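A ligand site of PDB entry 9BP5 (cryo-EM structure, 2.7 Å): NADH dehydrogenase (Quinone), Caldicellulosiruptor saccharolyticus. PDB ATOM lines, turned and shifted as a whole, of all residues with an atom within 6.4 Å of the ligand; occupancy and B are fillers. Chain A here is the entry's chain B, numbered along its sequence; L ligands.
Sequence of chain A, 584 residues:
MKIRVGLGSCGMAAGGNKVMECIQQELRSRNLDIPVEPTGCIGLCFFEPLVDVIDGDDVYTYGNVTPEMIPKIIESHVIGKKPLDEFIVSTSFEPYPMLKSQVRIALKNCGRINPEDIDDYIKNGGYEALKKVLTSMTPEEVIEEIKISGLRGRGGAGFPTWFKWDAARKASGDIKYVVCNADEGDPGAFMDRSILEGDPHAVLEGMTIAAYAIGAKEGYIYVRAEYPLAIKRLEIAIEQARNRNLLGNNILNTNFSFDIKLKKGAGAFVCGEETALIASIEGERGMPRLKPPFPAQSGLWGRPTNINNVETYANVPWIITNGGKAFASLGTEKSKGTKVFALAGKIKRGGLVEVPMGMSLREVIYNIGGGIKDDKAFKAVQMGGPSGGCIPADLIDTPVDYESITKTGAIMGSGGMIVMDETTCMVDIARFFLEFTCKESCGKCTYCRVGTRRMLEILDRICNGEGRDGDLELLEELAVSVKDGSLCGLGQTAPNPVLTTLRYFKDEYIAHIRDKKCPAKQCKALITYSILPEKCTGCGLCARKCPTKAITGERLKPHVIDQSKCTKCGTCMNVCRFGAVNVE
The backbone NH (N) of Cys 445 lies close to a sulfur (S4) of the ligand, at 3.4 Å.
The side-chain sulfur (SG) of Cys 445 is bound to an iron atom (FE2) of the ligand, at 2.3 Å.
A sulfur (S2) of the ligand lies close to the backbone NH of Cys 442 (3.5 Å).
An iron atom (FE1) of the ligand is bound by the side-chain sulfur of Cys 442, at 2.3 Å.
FE4 of the ligand is bound by SG of Cys 488, at 2.3 Å.
SG of Cys 448 is bound to FE3 of the ligand (2.3 Å).
OG of Ser 441 sits close to S4 of the ligand (3.6 Å).
N of Lys 444 lies close to S4 of the ligand (3.3 Å).
N of Gly 491 sits close to S1 of the ligand.
The backbone NH of Gly 443 lies close to a sulfur (S4) of the ligand (3.6 Å).
Merely in contact with the ligand: Ser 486, Leu 490 and Leu 487.
Hydrophobic or aromatic side chains within 4 Å of the ligand: Leu 487 and Leu 490.
Within 4 Å of the ligand: Ser 441, Cys 442, Gly 443, Lys 444, Cys 445, Cys 448, Ser 486, Leu 487, Cys 488, Leu 490 and Gly 491.
SG of Cys 445 lies close to N of Leu 487, at 3.7 Å.
The side-chain sulfur (SG) of Cys 442 sits close to the backbone NH (N) of Lys 444.
The side-chain sulfur (SG) of Cys 488 lies close to the backbone NH (N) of Leu 490 (3.2 Å).
SG of Cys 448 lies close to OG of Ser 441 (2.6 Å).
O of Pro 288 is in hydrogen-bond range of NZ of Lys 444 (2.9 Å).
The backbone carbonyl oxygen of Lys 444 sits at hydrogen-bond distance from the guanidinium group of Arg 449, at 3.2 Å.
The backbone carbonyl oxygen of Ser 486 lies close to the side-chain amide oxygen of Gln 492.
O of Leu 487 lies close to OE1 of Gln 492.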
ATOM      1  N   VAL A 270      -1.062  10.525  10.889  1.00  0.00           N
ATOM      2  CA  VAL A 270      -1.340  11.258  12.113  1.00  0.00           C
ATOM      3  C   VAL A 270      -0.202  11.108  13.107  1.00  0.00           C
ATOM      4  O   VAL A 270       0.073  12.030  13.880  1.00  0.00           O
ATOM      5  CB  VAL A 270      -2.689  10.807  12.716  1.00  0.00           C
ATOM      6  CG1 VAL A 270      -2.649   9.338  13.081  1.00  0.00           C
ATOM      7  CG2 VAL A 270      -3.039  11.643  13.916  1.00  0.00           C
ATOM      8  N   MET A 287      -3.610   8.847  18.915  1.00  0.00           N
ATOM      9  CA  MET A 287      -4.661   9.857  18.883  1.00  0.00           C
ATOM     10  C   MET A 287      -4.109  11.155  19.463  1.00  0.00           C
ATOM     11  O   MET A 287      -3.710  11.160  20.629  1.00  0.00           O
ATOM     12  CB  MET A 287      -5.873   9.402  19.675  1.00  0.00           C
ATOM     13  CG  MET A 287      -6.893   8.619  18.864  1.00  0.00           C
ATOM     14  SD  MET A 287      -8.479   8.495  19.702  1.00  0.00           S
ATOM     15  CE  MET A 287      -9.528   7.908  18.379  1.00  0.00           C
ATOM     16  N   PRO A 288      -4.062  12.239  18.696  1.00  0.00           N
ATOM     17  CA  PRO A 288      -3.482  13.478  19.208  1.00  0.00           C
ATOM     18  C   PRO A 288      -4.174  13.980  20.465  1.00  0.00           C
ATOM     19  O   PRO A 288      -5.399  13.914  20.581  1.00  0.00           O
ATOM     20  CB  PRO A 288      -3.669  14.457  18.045  1.00  0.00           C
ATOM     21  CG  PRO A 288      -3.633  13.592  16.856  1.00  0.00           C
ATOM     22  CD  PRO A 288      -4.335  12.327  17.257  1.00  0.00           C
ATOM     23  N   GLU A 440      -6.213   8.517   6.349  1.00  0.00           N
ATOM     24  CA  GLU A 440      -5.185   8.626   7.367  1.00  0.00           C
ATOM     25  C   GLU A 440      -5.600   9.481   8.558  1.00  0.00           C
ATOM     26  O   GLU A 440      -4.763   9.794   9.414  1.00  0.00           O
ATOM     27  CB  GLU A 440      -3.889   9.173   6.776  1.00  0.00           C
ATOM     28  CG  GLU A 440      -3.219   8.240   5.777  1.00  0.00           C
ATOM     29  CD  GLU A 440      -2.344   7.196   6.450  1.00  0.00           C
ATOM     30  OE1 GLU A 440      -1.398   7.574   7.172  1.00  0.00           O
ATOM     31  OE2 GLU A 440      -2.584   5.985   6.248  1.00  0.00           O
ATOM     32  N   SER A 441      -6.864   9.882   8.639  1.00  0.00           N
ATOM     33  CA  SER A 441      -7.339  10.655   9.774  1.00  0.00           C
ATOM     34  C   SER A 441      -7.535   9.743  10.987  1.00  0.00           C
ATOM     35  O   SER A 441      -7.944   8.584  10.864  1.00  0.00           O
ATOM     36  CB  SER A 441      -8.654  11.355   9.440  1.00  0.00           C
ATOM     37  OG  SER A 441      -9.066  12.188  10.507  1.00  0.00           O
ATOM     38  N   CYS A 442      -7.258  10.293  12.176  1.00  0.00           N
ATOM     39  CA  CYS A 442      -7.377   9.488  13.385  1.00  0.00           C
ATOM     40  C   CYS A 442      -8.824   9.272  13.794  1.00  0.00           C
ATOM     41  O   CYS A 442      -9.099   8.365  14.589  1.00  0.00           O
ATOM     42  CB  CYS A 442      -6.609  10.134  14.537  1.00  0.00           C
ATOM     43  SG  CYS A 442      -7.596  11.213  15.571  1.00  0.00           S
ATOM     44  N   GLY A 443      -9.745  10.076  13.271  1.00  0.00           N
ATOM     45  CA  GLY A 443     -11.160   9.881  13.557  1.00  0.00           C
ATOM     46  C   GLY A 443     -11.563  10.134  14.988  1.00  0.00           C
ATOM     47  O   GLY A 443     -12.341   9.349  15.550  1.00  0.00           O
ATOM     48  N   LYS A 444     -11.065  11.202  15.600  1.00  0.00           N
ATOM     49  CA  LYS A 444     -11.450  11.574  16.957  1.00  0.00           C
ATOM     50  C   LYS A 444     -12.443  12.732  16.978  1.00  0.00           C
ATOM     51  O   LYS A 444     -13.446  12.675  17.685  1.00  0.00           O
ATOM     52  CB  LYS A 444     -10.219  11.930  17.788  1.00  0.00           C
ATOM     53  CG  LYS A 444     -10.531  12.712  19.054  1.00  0.00           C
ATOM     54  CD  LYS A 444      -9.268  13.204  19.747  1.00  0.00           C
ATOM     55  CE  LYS A 444      -8.406  12.046  20.212  1.00  0.00           C
ATOM     56  NZ  LYS A 444      -7.662  12.367  21.458  1.00  0.00           N
ATOM     57  N   CYS A 445     -12.180  13.784  16.207  1.00  0.00           N
ATOM     58  CA  CYS A 445     -13.045  14.951  16.165  1.00  0.00           C
ATOM     59  C   CYS A 445     -13.873  14.947  14.884  1.00  0.00           C
ATOM     60  O   CYS A 445     -13.381  14.616  13.813  1.00  0.00           O
ATOM     61  CB  CYS A 445     -12.234  16.247  16.271  1.00  0.00           C
ATOM     62  SG  CYS A 445     -11.194  16.620  14.875  1.00  0.00           S
ATOM     63  N   THR A 446     -15.153  15.314  15.021  1.00  0.00           N
ATOM     64  CA  THR A 446     -16.099  15.215  13.919  1.00  0.00           C
ATOM     65  C   THR A 446     -15.728  16.111  12.744  1.00  0.00           C
ATOM     66  O   THR A 446     -16.148  15.838  11.618  1.00  0.00           O
ATOM     67  CB  THR A 446     -17.505  15.573  14.390  1.00  0.00           C
ATOM     68  OG1 THR A 446     -18.365  15.720  13.266  1.00  0.00           O
ATOM     69  CG2 THR A 446     -17.491  16.867  15.175  1.00  0.00           C
ATOM     70  N   TYR A 447     -14.971  17.189  12.978  1.00  0.00           N
ATOM     71  CA  TYR A 447     -14.621  18.091  11.890  1.00  0.00           C
ATOM     72  C   TYR A 447     -13.682  17.410  10.904  1.00  0.00           C
ATOM     73  O   TYR A 447     -13.883  17.494   9.683  1.00  0.00           O
ATOM     74  CB  TYR A 447     -13.987  19.344  12.462  1.00  0.00           C
ATOM     75  CG  TYR A 447     -14.969  20.475  12.615  1.00  0.00           C
ATOM     76  CD1 TYR A 447     -15.921  20.716  11.637  1.00  0.00           C
ATOM     77  CD2 TYR A 447     -14.982  21.264  13.751  1.00  0.00           C
ATOM     78  CE1 TYR A 447     -16.819  21.740  11.775  1.00  0.00           C
ATOM     79  CE2 TYR A 447     -15.889  22.296  13.895  1.00  0.00           C
ATOM     80  CZ  TYR A 447     -16.813  22.520  12.902  1.00  0.00           C
ATOM     81  OH  TYR A 447     -17.724  23.547  13.034  1.00  0.00           O
ATOM     82  N   CYS A 448     -12.650  16.732  11.400  1.00  0.00           N
ATOM     83  CA  CYS A 448     -11.792  15.929  10.526  1.00  0.00           C
ATOM     84  C   CYS A 448     -12.438  14.611  10.152  1.00  0.00           C
ATOM     85  O   CYS A 448     -12.238  14.119   9.037  1.00  0.00           O
ATOM     86  CB  CYS A 448     -10.449  15.681  11.196  1.00  0.00           C
ATOM     87  SG  CYS A 448      -9.262  14.753  10.213  1.00  0.00           S
ATOM     88  N   ARG A 449     -13.226  14.025  11.058  1.00  0.00           N
ATOM     89  CA  ARG A 449     -13.758  12.685  10.815  1.00  0.00           C
ATOM     90  C   ARG A 449     -14.862  12.705   9.763  1.00  0.00           C
ATOM     91  O   ARG A 449     -14.929  11.814   8.917  1.00  0.00           O
ATOM     92  CB  ARG A 449     -14.275  12.090  12.122  1.00  0.00           C
ATOM     93  CG  ARG A 449     -14.425  10.590  12.113  1.00  0.00           C
ATOM     94  CD  ARG A 449     -14.787  10.068  13.481  1.00  0.00           C
ATOM     95  NE  ARG A 449     -16.167  10.406  13.846  1.00  0.00           N
ATOM     96  CZ  ARG A 449     -16.495  11.340  14.723  1.00  0.00           C
ATOM     97  NH1 ARG A 449     -15.586  12.057  15.351  1.00  0.00           N
ATOM     98  NH2 ARG A 449     -17.784  11.571  14.969  1.00  0.00           N
ATOM     99  N   SER A 486     -11.008  21.841  13.614  1.00  0.00           N
ATOM    100  CA  SER A 486     -10.417  20.555  13.910  1.00  0.00           C
ATOM    101  C   SER A 486      -9.428  20.671  15.066  1.00  0.00           C
ATOM    102  O   SER A 486      -8.994  21.755  15.454  1.00  0.00           O
ATOM    103  CB  SER A 486      -9.717  19.988  12.676  1.00  0.00           C
ATOM    104  OG  SER A 486     -10.539  20.141  11.534  1.00  0.00           O
ATOM    105  N   LEU A 487      -9.075  19.516  15.641  1.00  0.00           N
ATOM    106  CA  LEU A 487      -8.219  19.478  16.816  1.00  0.00           C
ATOM    107  C   LEU A 487      -6.751  19.624  16.438  1.00  0.00           C
ATOM    108  O   LEU A 487      -6.079  20.583  16.853  1.00  0.00           O
ATOM    109  CB  LEU A 487      -8.441  18.174  17.584  1.00  0.00           C
ATOM    110  CG  LEU A 487      -8.327  18.180  19.107  1.00  0.00           C
ATOM    111  CD1 LEU A 487      -8.753  16.831  19.658  1.00  0.00           C
ATOM    112  CD2 LEU A 487      -6.919  18.519  19.556  1.00  0.00           C
ATOM    113  N   CYS A 488      -6.226  18.690  15.657  1.00  0.00           N
ATOM    114  CA  CYS A 488      -4.808  18.638  15.335  1.00  0.00           C
ATOM    115  C   CYS A 488      -4.580  19.206  13.932  1.00  0.00           C
ATOM    116  O   CYS A 488      -5.503  19.623  13.243  1.00  0.00           O
ATOM    117  CB  CYS A 488      -4.287  17.213  15.437  1.00  0.00           C
ATOM    118  SG  CYS A 488      -4.400  16.275  13.914  1.00  0.00           S
ATOM    119  N   GLY A 489      -3.320  19.214  13.521  1.00  0.00           N
ATOM    120  CA  GLY A 489      -2.947  19.830  12.261  1.00  0.00           C
ATOM    121  C   GLY A 489      -3.304  19.028  11.033  1.00  0.00           C
ATOM    122  O   GLY A 489      -3.220  19.570   9.927  1.00  0.00           O
ATOM    123  N   LEU A 490      -3.683  17.763  11.192  1.00  0.00           N
ATOM    124  CA  LEU A 490      -4.138  16.989  10.037  1.00  0.00           C
ATOM    125  C   LEU A 490      -5.428  17.548   9.473  1.00  0.00           C
ATOM    126  O   LEU A 490      -5.578  17.662   8.253  1.00  0.00           O
ATOM    127  CB  LEU A 490      -4.299  15.523  10.420  1.00  0.00           C
ATOM    128  CG  LEU A 490      -4.823  14.543   9.368  1.00  0.00           C
ATOM    129  CD1 LEU A 490      -4.211  14.805   8.008  1.00  0.00           C
ATOM    130  CD2 LEU A 490      -4.513  13.126   9.800  1.00  0.00           C
ATOM    131  N   GLY A 491      -6.381  17.911  10.339  1.00  0.00           N
ATOM    132  CA  GLY A 491      -7.639  18.461   9.865  1.00  0.00           C
ATOM    133  C   GLY A 491      -7.592  19.943   9.609  1.00  0.00           C
ATOM    134  O   GLY A 491      -8.339  20.450   8.768  1.00  0.00           O
ATOM    135  N   GLN A 492      -6.736  20.670  10.322  1.00  0.00           N
ATOM    136  CA  GLN A 492      -6.615  22.108  10.106  1.00  0.00           C
ATOM    137  C   GLN A 492      -5.863  22.433   8.829  1.00  0.00           C
ATOM    138  O   GLN A 492      -5.897  23.578   8.382  1.00  0.00           O
ATOM    139  CB  GLN A 492      -5.931  22.764  11.295  1.00  0.00           C
ATOM    140  CG  GLN A 492      -6.566  22.438  12.632  1.00  0.00           C
ATOM    141  CD  GLN A 492      -5.768  22.965  13.800  1.00  0.00           C
ATOM    142  OE1 GLN A 492      -6.336  23.336  14.818  1.00  0.00           O
ATOM    143  NE2 GLN A 492      -4.458  23.007  13.651  1.00  0.00           N
HETATM  144 FE1  LIG L   1      -7.852  13.235  14.613  1.00  0.00          FE
HETATM  145 FE2  LIG L   1      -9.198  15.607  14.639  1.00  0.00          FE
HETATM  146 FE3  LIG L   1      -8.353  14.549  12.271  1.00  0.00          FE
HETATM  147 FE4  LIG L   1      -6.527  15.545  14.047  1.00  0.00          FE
HETATM  148  S1  LIG L   1      -8.147  16.714  12.945  1.00  0.00           S
HETATM  149  S2  LIG L   1      -6.390  13.589  12.906  1.00  0.00           S
HETATM  150  S3  LIG L   1      -7.503  14.974  16.026  1.00  0.00           S
HETATM  151  S4  LIG L   1      -9.892  13.662  13.684  1.00  0.00           S
